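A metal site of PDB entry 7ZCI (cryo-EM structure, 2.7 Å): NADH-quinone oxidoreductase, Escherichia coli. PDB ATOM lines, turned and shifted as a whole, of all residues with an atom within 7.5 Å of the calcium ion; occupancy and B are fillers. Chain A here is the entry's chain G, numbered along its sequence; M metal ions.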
ATOM      1  N   GLU A 615      18.789 -24.939  30.742  1.00  0.00           N
ATOM      2  CA  GLU A 615      18.687 -26.259  30.121  1.00  0.00           C
ATOM      3  C   GLU A 615      18.876 -26.214  28.614  1.00  0.00           C
ATOM      4  O   GLU A 615      18.508 -27.164  27.925  1.00  0.00           O
ATOM      5  CB  GLU A 615      17.347 -26.894  30.452  1.00  0.00           C
ATOM      6  CG  GLU A 615      16.993 -26.878  31.903  1.00  0.00           C
ATOM      7  CD  GLU A 615      15.858 -25.955  32.218  1.00  0.00           C
ATOM      8  OE1 GLU A 615      15.370 -25.270  31.299  1.00  0.00           O
ATOM      9  OE2 GLU A 615      15.440 -25.907  33.395  1.00  0.00           O
ATOM     10  N   SER A 616      19.434 -25.134  28.082  1.00  0.00           N
ATOM     11  CA  SER A 616      19.520 -24.995  26.642  1.00  0.00           C
ATOM     12  C   SER A 616      20.809 -24.289  26.266  1.00  0.00           C
ATOM     13  O   SER A 616      21.451 -23.621  27.087  1.00  0.00           O
ATOM     14  CB  SER A 616      18.315 -24.231  26.075  1.00  0.00           C
ATOM     15  OG  SER A 616      18.124 -23.003  26.737  1.00  0.00           O
ATOM     16  N   ASP A 617      21.187 -24.437  25.012  1.00  0.00           N
ATOM     17  CA  ASP A 617      22.267 -23.687  24.403  1.00  0.00           C
ATOM     18  C   ASP A 617      21.675 -22.703  23.406  1.00  0.00           C
ATOM     19  O   ASP A 617      20.552 -22.880  22.929  1.00  0.00           O
ATOM     20  CB  ASP A 617      23.253 -24.605  23.686  1.00  0.00           C
ATOM     21  CG  ASP A 617      23.399 -25.945  24.358  1.00  0.00           C
ATOM     22  OD1 ASP A 617      24.169 -26.043  25.321  1.00  0.00           O
ATOM     23  OD2 ASP A 617      22.719 -26.898  23.933  1.00  0.00           O
ATOM     24  N   PHE A 631      25.531 -21.608  27.177  1.00  0.00           N
ATOM     25  CA  PHE A 631      25.690 -23.048  27.174  1.00  0.00           C
ATOM     26  C   PHE A 631      24.757 -23.653  28.211  1.00  0.00           C
ATOM     27  O   PHE A 631      24.415 -23.020  29.206  1.00  0.00           O
ATOM     28  CB  PHE A 631      27.150 -23.429  27.484  1.00  0.00           C
ATOM     29  CG  PHE A 631      28.149 -22.922  26.473  1.00  0.00           C
ATOM     30  CD1 PHE A 631      28.586 -21.614  26.486  1.00  0.00           C
ATOM     31  CD2 PHE A 631      28.650 -23.771  25.514  1.00  0.00           C
ATOM     32  CE1 PHE A 631      29.480 -21.159  25.552  1.00  0.00           C
ATOM     33  CE2 PHE A 631      29.550 -23.324  24.581  1.00  0.00           C
ATOM     34  CZ  PHE A 631      29.972 -22.025  24.605  1.00  0.00           C
ATOM     35  N   GLN A 632      24.333 -24.885  27.950  1.00  0.00           N
ATOM     36  CA  GLN A 632      23.419 -25.580  28.850  1.00  0.00           C
ATOM     37  C   GLN A 632      24.113 -25.909  30.166  1.00  0.00           C
ATOM     38  O   GLN A 632      25.251 -26.384  30.169  1.00  0.00           O
ATOM     39  CB  GLN A 632      22.895 -26.847  28.182  1.00  0.00           C
ATOM     40  CG  GLN A 632      22.031 -27.732  29.051  1.00  0.00           C
ATOM     41  CD  GLN A 632      21.422 -28.875  28.281  1.00  0.00           C
ATOM     42  OE1 GLN A 632      21.576 -28.966  27.073  1.00  0.00           O
ATOM     43  NE2 GLN A 632      20.703 -29.741  28.972  1.00  0.00           N
ATOM     44  N   TYR A 634      22.656 -27.887  32.849  1.00  0.00           N
ATOM     45  CA  TYR A 634      22.387 -29.242  33.284  1.00  0.00           C
ATOM     46  C   TYR A 634      21.419 -29.911  32.333  1.00  0.00           C
ATOM     47  O   TYR A 634      20.679 -29.259  31.590  1.00  0.00           O
ATOM     48  CB  TYR A 634      21.822 -29.293  34.701  1.00  0.00           C
ATOM     49  CG  TYR A 634      20.400 -28.790  34.860  1.00  0.00           C
ATOM     50  CD1 TYR A 634      20.101 -27.441  34.829  1.00  0.00           C
ATOM     51  CD2 TYR A 634      19.360 -29.687  35.046  1.00  0.00           C
ATOM     52  CE1 TYR A 634      18.809 -26.996  34.964  1.00  0.00           C
ATOM     53  CE2 TYR A 634      18.067 -29.255  35.188  1.00  0.00           C
ATOM     54  CZ  TYR A 634      17.794 -27.914  35.147  1.00  0.00           C
ATOM     55  OH  TYR A 634      16.500 -27.482  35.289  1.00  0.00           O
ATOM     56  N   ASP A 635      21.434 -31.239  32.361  1.00  0.00           N
ATOM     57  CA  ASP A 635      20.437 -32.033  31.654  1.00  0.00           C
ATOM     58  C   ASP A 635      19.211 -32.200  32.531  1.00  0.00           C
ATOM     59  O   ASP A 635      19.331 -32.752  33.641  1.00  0.00           O
ATOM     60  CB  ASP A 635      21.013 -33.383  31.283  1.00  0.00           C
ATOM     61  CG  ASP A 635      20.007 -34.280  30.592  1.00  0.00           C
ATOM     62  OD1 ASP A 635      19.321 -33.810  29.666  1.00  0.00           O
ATOM     63  OD2 ASP A 635      19.893 -35.457  30.987  1.00  0.00           O
ATOM     64  N   GLU A 647      15.557 -28.057  23.794  1.00  0.00           N
ATOM     65  CA  GLU A 647      15.780 -26.732  23.275  1.00  0.00           C
ATOM     66  C   GLU A 647      14.720 -26.379  22.249  1.00  0.00           C
ATOM     67  O   GLU A 647      14.204 -27.252  21.537  1.00  0.00           O
ATOM     68  CB  GLU A 647      17.160 -26.622  22.640  1.00  0.00           C
ATOM     69  CG  GLU A 647      18.313 -26.833  23.590  1.00  0.00           C
ATOM     70  CD  GLU A 647      18.751 -28.269  23.714  1.00  0.00           C
ATOM     71  OE1 GLU A 647      18.108 -29.155  23.118  1.00  0.00           O
ATOM     72  OE2 GLU A 647      19.744 -28.524  24.424  1.00  0.00           O
ATOM     73  N   TRP A 649      14.958 -24.547  19.497  1.00  0.00           N
ATOM     74  CA  TRP A 649      15.430 -24.801  18.137  1.00  0.00           C
ATOM     75  C   TRP A 649      15.416 -26.291  17.820  1.00  0.00           C
ATOM     76  O   TRP A 649      15.150 -26.671  16.678  1.00  0.00           O
ATOM     77  CB  TRP A 649      16.831 -24.241  17.933  1.00  0.00           C
ATOM     78  CG  TRP A 649      17.821 -24.616  18.980  1.00  0.00           C
ATOM     79  CD1 TRP A 649      18.144 -23.904  20.094  1.00  0.00           C
ATOM     80  CD2 TRP A 649      18.639 -25.783  19.008  1.00  0.00           C
ATOM     81  NE1 TRP A 649      19.109 -24.548  20.807  1.00  0.00           N
ATOM     82  CE2 TRP A 649      19.431 -25.718  20.161  1.00  0.00           C
ATOM     83  CE3 TRP A 649      18.783 -26.884  18.150  1.00  0.00           C
ATOM     84  CZ2 TRP A 649      20.347 -26.704  20.492  1.00  0.00           C
ATOM     85  CZ3 TRP A 649      19.690 -27.862  18.494  1.00  0.00           C
ATOM     86  CH2 TRP A 649      20.452 -27.769  19.649  1.00  0.00           C
ATOM     87  N   ARG A 650      15.671 -27.144  18.813  1.00  0.00           N
ATOM     88  CA  ARG A 650      15.612 -28.581  18.589  1.00  0.00           C
ATOM     89  C   ARG A 650      14.175 -29.038  18.339  1.00  0.00           C
ATOM     90  O   ARG A 650      13.936 -29.816  17.408  1.00  0.00           O
ATOM     91  CB  ARG A 650      16.233 -29.296  19.797  1.00  0.00           C
ATOM     92  CG  ARG A 650      16.148 -30.800  19.776  1.00  0.00           C
ATOM     93  CD  ARG A 650      17.215 -31.414  20.643  1.00  0.00           C
ATOM     94  NE  ARG A 650      18.488 -31.561  19.941  1.00  0.00           N
ATOM     95  CZ  ARG A 650      19.662 -31.154  20.393  1.00  0.00           C
ATOM     96  NH1 ARG A 650      19.781 -30.531  21.553  1.00  0.00           N
ATOM     97  NH2 ARG A 650      20.746 -31.389  19.667  1.00  0.00           N
ATOM     98  N   LEU A 669      23.460 -28.270  17.520  1.00  0.00           N
ATOM     99  CA  LEU A 669      23.450 -26.811  17.621  1.00  0.00           C
ATOM    100  C   LEU A 669      24.279 -26.165  16.520  1.00  0.00           C
ATOM    101  O   LEU A 669      23.887 -25.133  15.958  1.00  0.00           O
ATOM    102  CB  LEU A 669      23.961 -26.377  18.993  1.00  0.00           C
ATOM    103  CG  LEU A 669      24.277 -24.886  19.173  1.00  0.00           C
ATOM    104  CD1 LEU A 669      23.016 -24.054  19.182  1.00  0.00           C
ATOM    105  CD2 LEU A 669      25.100 -24.653  20.426  1.00  0.00           C
ATOM    106  N   ARG A 704      32.232 -29.031  33.107  1.00  0.00           N
ATOM    107  CA  ARG A 704      31.180 -28.212  33.698  1.00  0.00           C
ATOM    108  C   ARG A 704      31.241 -28.164  35.219  1.00  0.00           C
ATOM    109  O   ARG A 704      30.732 -27.219  35.810  1.00  0.00           O
ATOM    110  CB  ARG A 704      29.802 -28.722  33.285  1.00  0.00           C
ATOM    111  CG  ARG A 704      29.281 -28.117  32.008  1.00  0.00           C
ATOM    112  CD  ARG A 704      27.889 -28.634  31.716  1.00  0.00           C
ATOM    113  NE  ARG A 704      27.299 -28.029  30.533  1.00  0.00           N
ATOM    114  CZ  ARG A 704      27.358 -28.534  29.313  1.00  0.00           C
ATOM    115  NH1 ARG A 704      27.988 -29.670  29.069  1.00  0.00           N
ATOM    116  NH2 ARG A 704      26.771 -27.893  28.306  1.00  0.00           N
ATOM    117  N   GLN A 728      25.187 -37.041  27.640  1.00  0.00           N
ATOM    118  CA  GLN A 728      26.083 -36.676  26.566  1.00  0.00           C
ATOM    119  C   GLN A 728      25.741 -35.297  26.034  1.00  0.00           C
ATOM    120  O   GLN A 728      24.570 -34.915  25.969  1.00  0.00           O
ATOM    121  CB  GLN A 728      26.025 -37.720  25.442  1.00  0.00           C
ATOM    122  CG  GLN A 728      26.906 -38.974  25.590  1.00  0.00           C
ATOM    123  CD  GLN A 728      28.211 -38.803  26.367  1.00  0.00           C
ATOM    124  OE1 GLN A 728      28.222 -38.690  27.604  1.00  0.00           O
ATOM    125  NE2 GLN A 728      29.327 -38.780  25.650  1.00  0.00           N
ATOM    126  N   ASP A 729      26.765 -34.543  25.681  1.00  0.00           N
ATOM    127  CA  ASP A 729      26.603 -33.198  25.136  1.00  0.00           C
ATOM    128  C   ASP A 729      27.119 -33.221  23.706  1.00  0.00           C
ATOM    129  O   ASP A 729      28.328 -33.170  23.473  1.00  0.00           O
ATOM    130  CB  ASP A 729      27.330 -32.171  25.987  1.00  0.00           C
ATOM    131  CG  ASP A 729      26.895 -30.755  25.688  1.00  0.00           C
ATOM    132  OD1 ASP A 729      25.690 -30.518  25.539  1.00  0.00           O
ATOM    133  OD2 ASP A 729      27.770 -29.875  25.603  1.00  0.00           O
ATOM    134  N   ILE A 730      26.196 -33.292  22.740  1.00  0.00           N
ATOM    135  CA  ILE A 730      26.582 -33.207  21.336  1.00  0.00           C
ATOM    136  C   ILE A 730      26.565 -31.780  20.825  1.00  0.00           C
ATOM    137  O   ILE A 730      27.113 -31.514  19.752  1.00  0.00           O
ATOM    138  CB  ILE A 730      25.653 -34.061  20.453  1.00  0.00           C
ATOM    139  CG1 ILE A 730      24.224 -33.538  20.510  1.00  0.00           C
ATOM    140  CG2 ILE A 730      25.702 -35.510  20.898  1.00  0.00           C
ATOM    141  CD1 ILE A 730      23.332 -34.047  19.422  1.00  0.00           C
ATOM    142  N   ASP A 731      25.991 -30.849  21.575  1.00  0.00           N
ATOM    143  CA  ASP A 731      25.802 -29.494  21.076  1.00  0.00           C
ATOM    144  C   ASP A 731      27.031 -28.621  21.293  1.00  0.00           C
ATOM    145  O   ASP A 731      27.354 -27.797  20.441  1.00  0.00           O
ATOM    146  CB  ASP A 731      24.577 -28.862  21.731  1.00  0.00           C
ATOM    147  CG  ASP A 731      23.296 -29.547  21.342  1.00  0.00           C
ATOM    148  OD1 ASP A 731      23.194 -29.986  20.183  1.00  0.00           O
ATOM    149  OD2 ASP A 731      22.400 -29.644  22.192  1.00  0.00           O
ATOM    150  N   THR A 732      27.711 -28.774  22.423  1.00  0.00           N
ATOM    151  CA  THR A 732      28.790 -27.867  22.782  1.00  0.00           C
ATOM    152  C   THR A 732      30.066 -28.651  23.082  1.00  0.00           C
ATOM    153  O   THR A 732      30.082 -29.884  23.076  1.00  0.00           O
ATOM    154  CB  THR A 732      28.450 -26.995  24.002  1.00  0.00           C
ATOM    155  OG1 THR A 732      28.565 -27.774  25.198  1.00  0.00           O
ATOM    156  CG2 THR A 732      27.050 -26.447  23.899  1.00  0.00           C
ATOM    157  N   PHE A 736      29.280 -32.870  30.638  1.00  0.00           N
ATOM    158  CA  PHE A 736      28.465 -32.829  31.843  1.00  0.00           C
ATOM    159  C   PHE A 736      29.108 -33.612  32.975  1.00  0.00           C
ATOM    160  O   PHE A 736      28.455 -34.466  33.580  1.00  0.00           O
ATOM    161  CB  PHE A 736      27.074 -33.391  31.571  1.00  0.00           C
ATOM    162  CG  PHE A 736      26.160 -32.444  30.834  1.00  0.00           C
ATOM    163  CD1 PHE A 736      25.568 -31.388  31.498  1.00  0.00           C
ATOM    164  CD2 PHE A 736      25.899 -32.622  29.497  1.00  0.00           C
ATOM    165  CE1 PHE A 736      24.733 -30.523  30.834  1.00  0.00           C
ATOM    166  CE2 PHE A 736      25.060 -31.761  28.825  1.00  0.00           C
ATOM    167  CZ  PHE A 736      24.478 -30.710  29.497  1.00  0.00           C
HETATM  168 CA    CA M   1      22.102 -29.153  24.662  1.00  0.00          CA
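N of Gln 632 lies within hydrogen-bond range of O of Ser 616, 3.3 Å away. The guanidinium group (NH1) of Arg 650 is in salt-bridge range of the side-chain carboxylate (OE1) of Glu 647, at 2.7 Å. NH1 of Arg 704 is in salt-bridge range of OD2 of Asp 729 (3.5 Å). O of Asp 617 is in hydrogen-bond range of NE1 of Trp 649 (3.1 Å). OD1 of Asp 731 is in salt-bridge range of NH2 of Arg 650 (2.9 Å). O of Tyr 634 sits at hydrogen-bond distance from NE2 of Gln 632, 2.7 Å away. The side-chain carboxylate (OD2) of Asp 729 lies close to the backbone NH (N) of Thr 732, at 3.4 Å. OD1 of Asp 731 lies within hydrogen-bond range of N of Leu 669 (3.2 Å).
The calcium ion is bound by the side-chain carboxylate (OD2) of Asp 617 (2.4 Å), the side-chain carboxylate (OE2) of Glu 647 (2.5 Å), the side-chain amide oxygen (OE1) of Gln 632 (2.5 Å) and the side-chain carboxylate (OD2) of Asp 731 (2.5 Å). The calcium ion has four donor atoms within binding distance.
OD1 of Asp 729 touches the calcium ion, 3.9 Å away.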
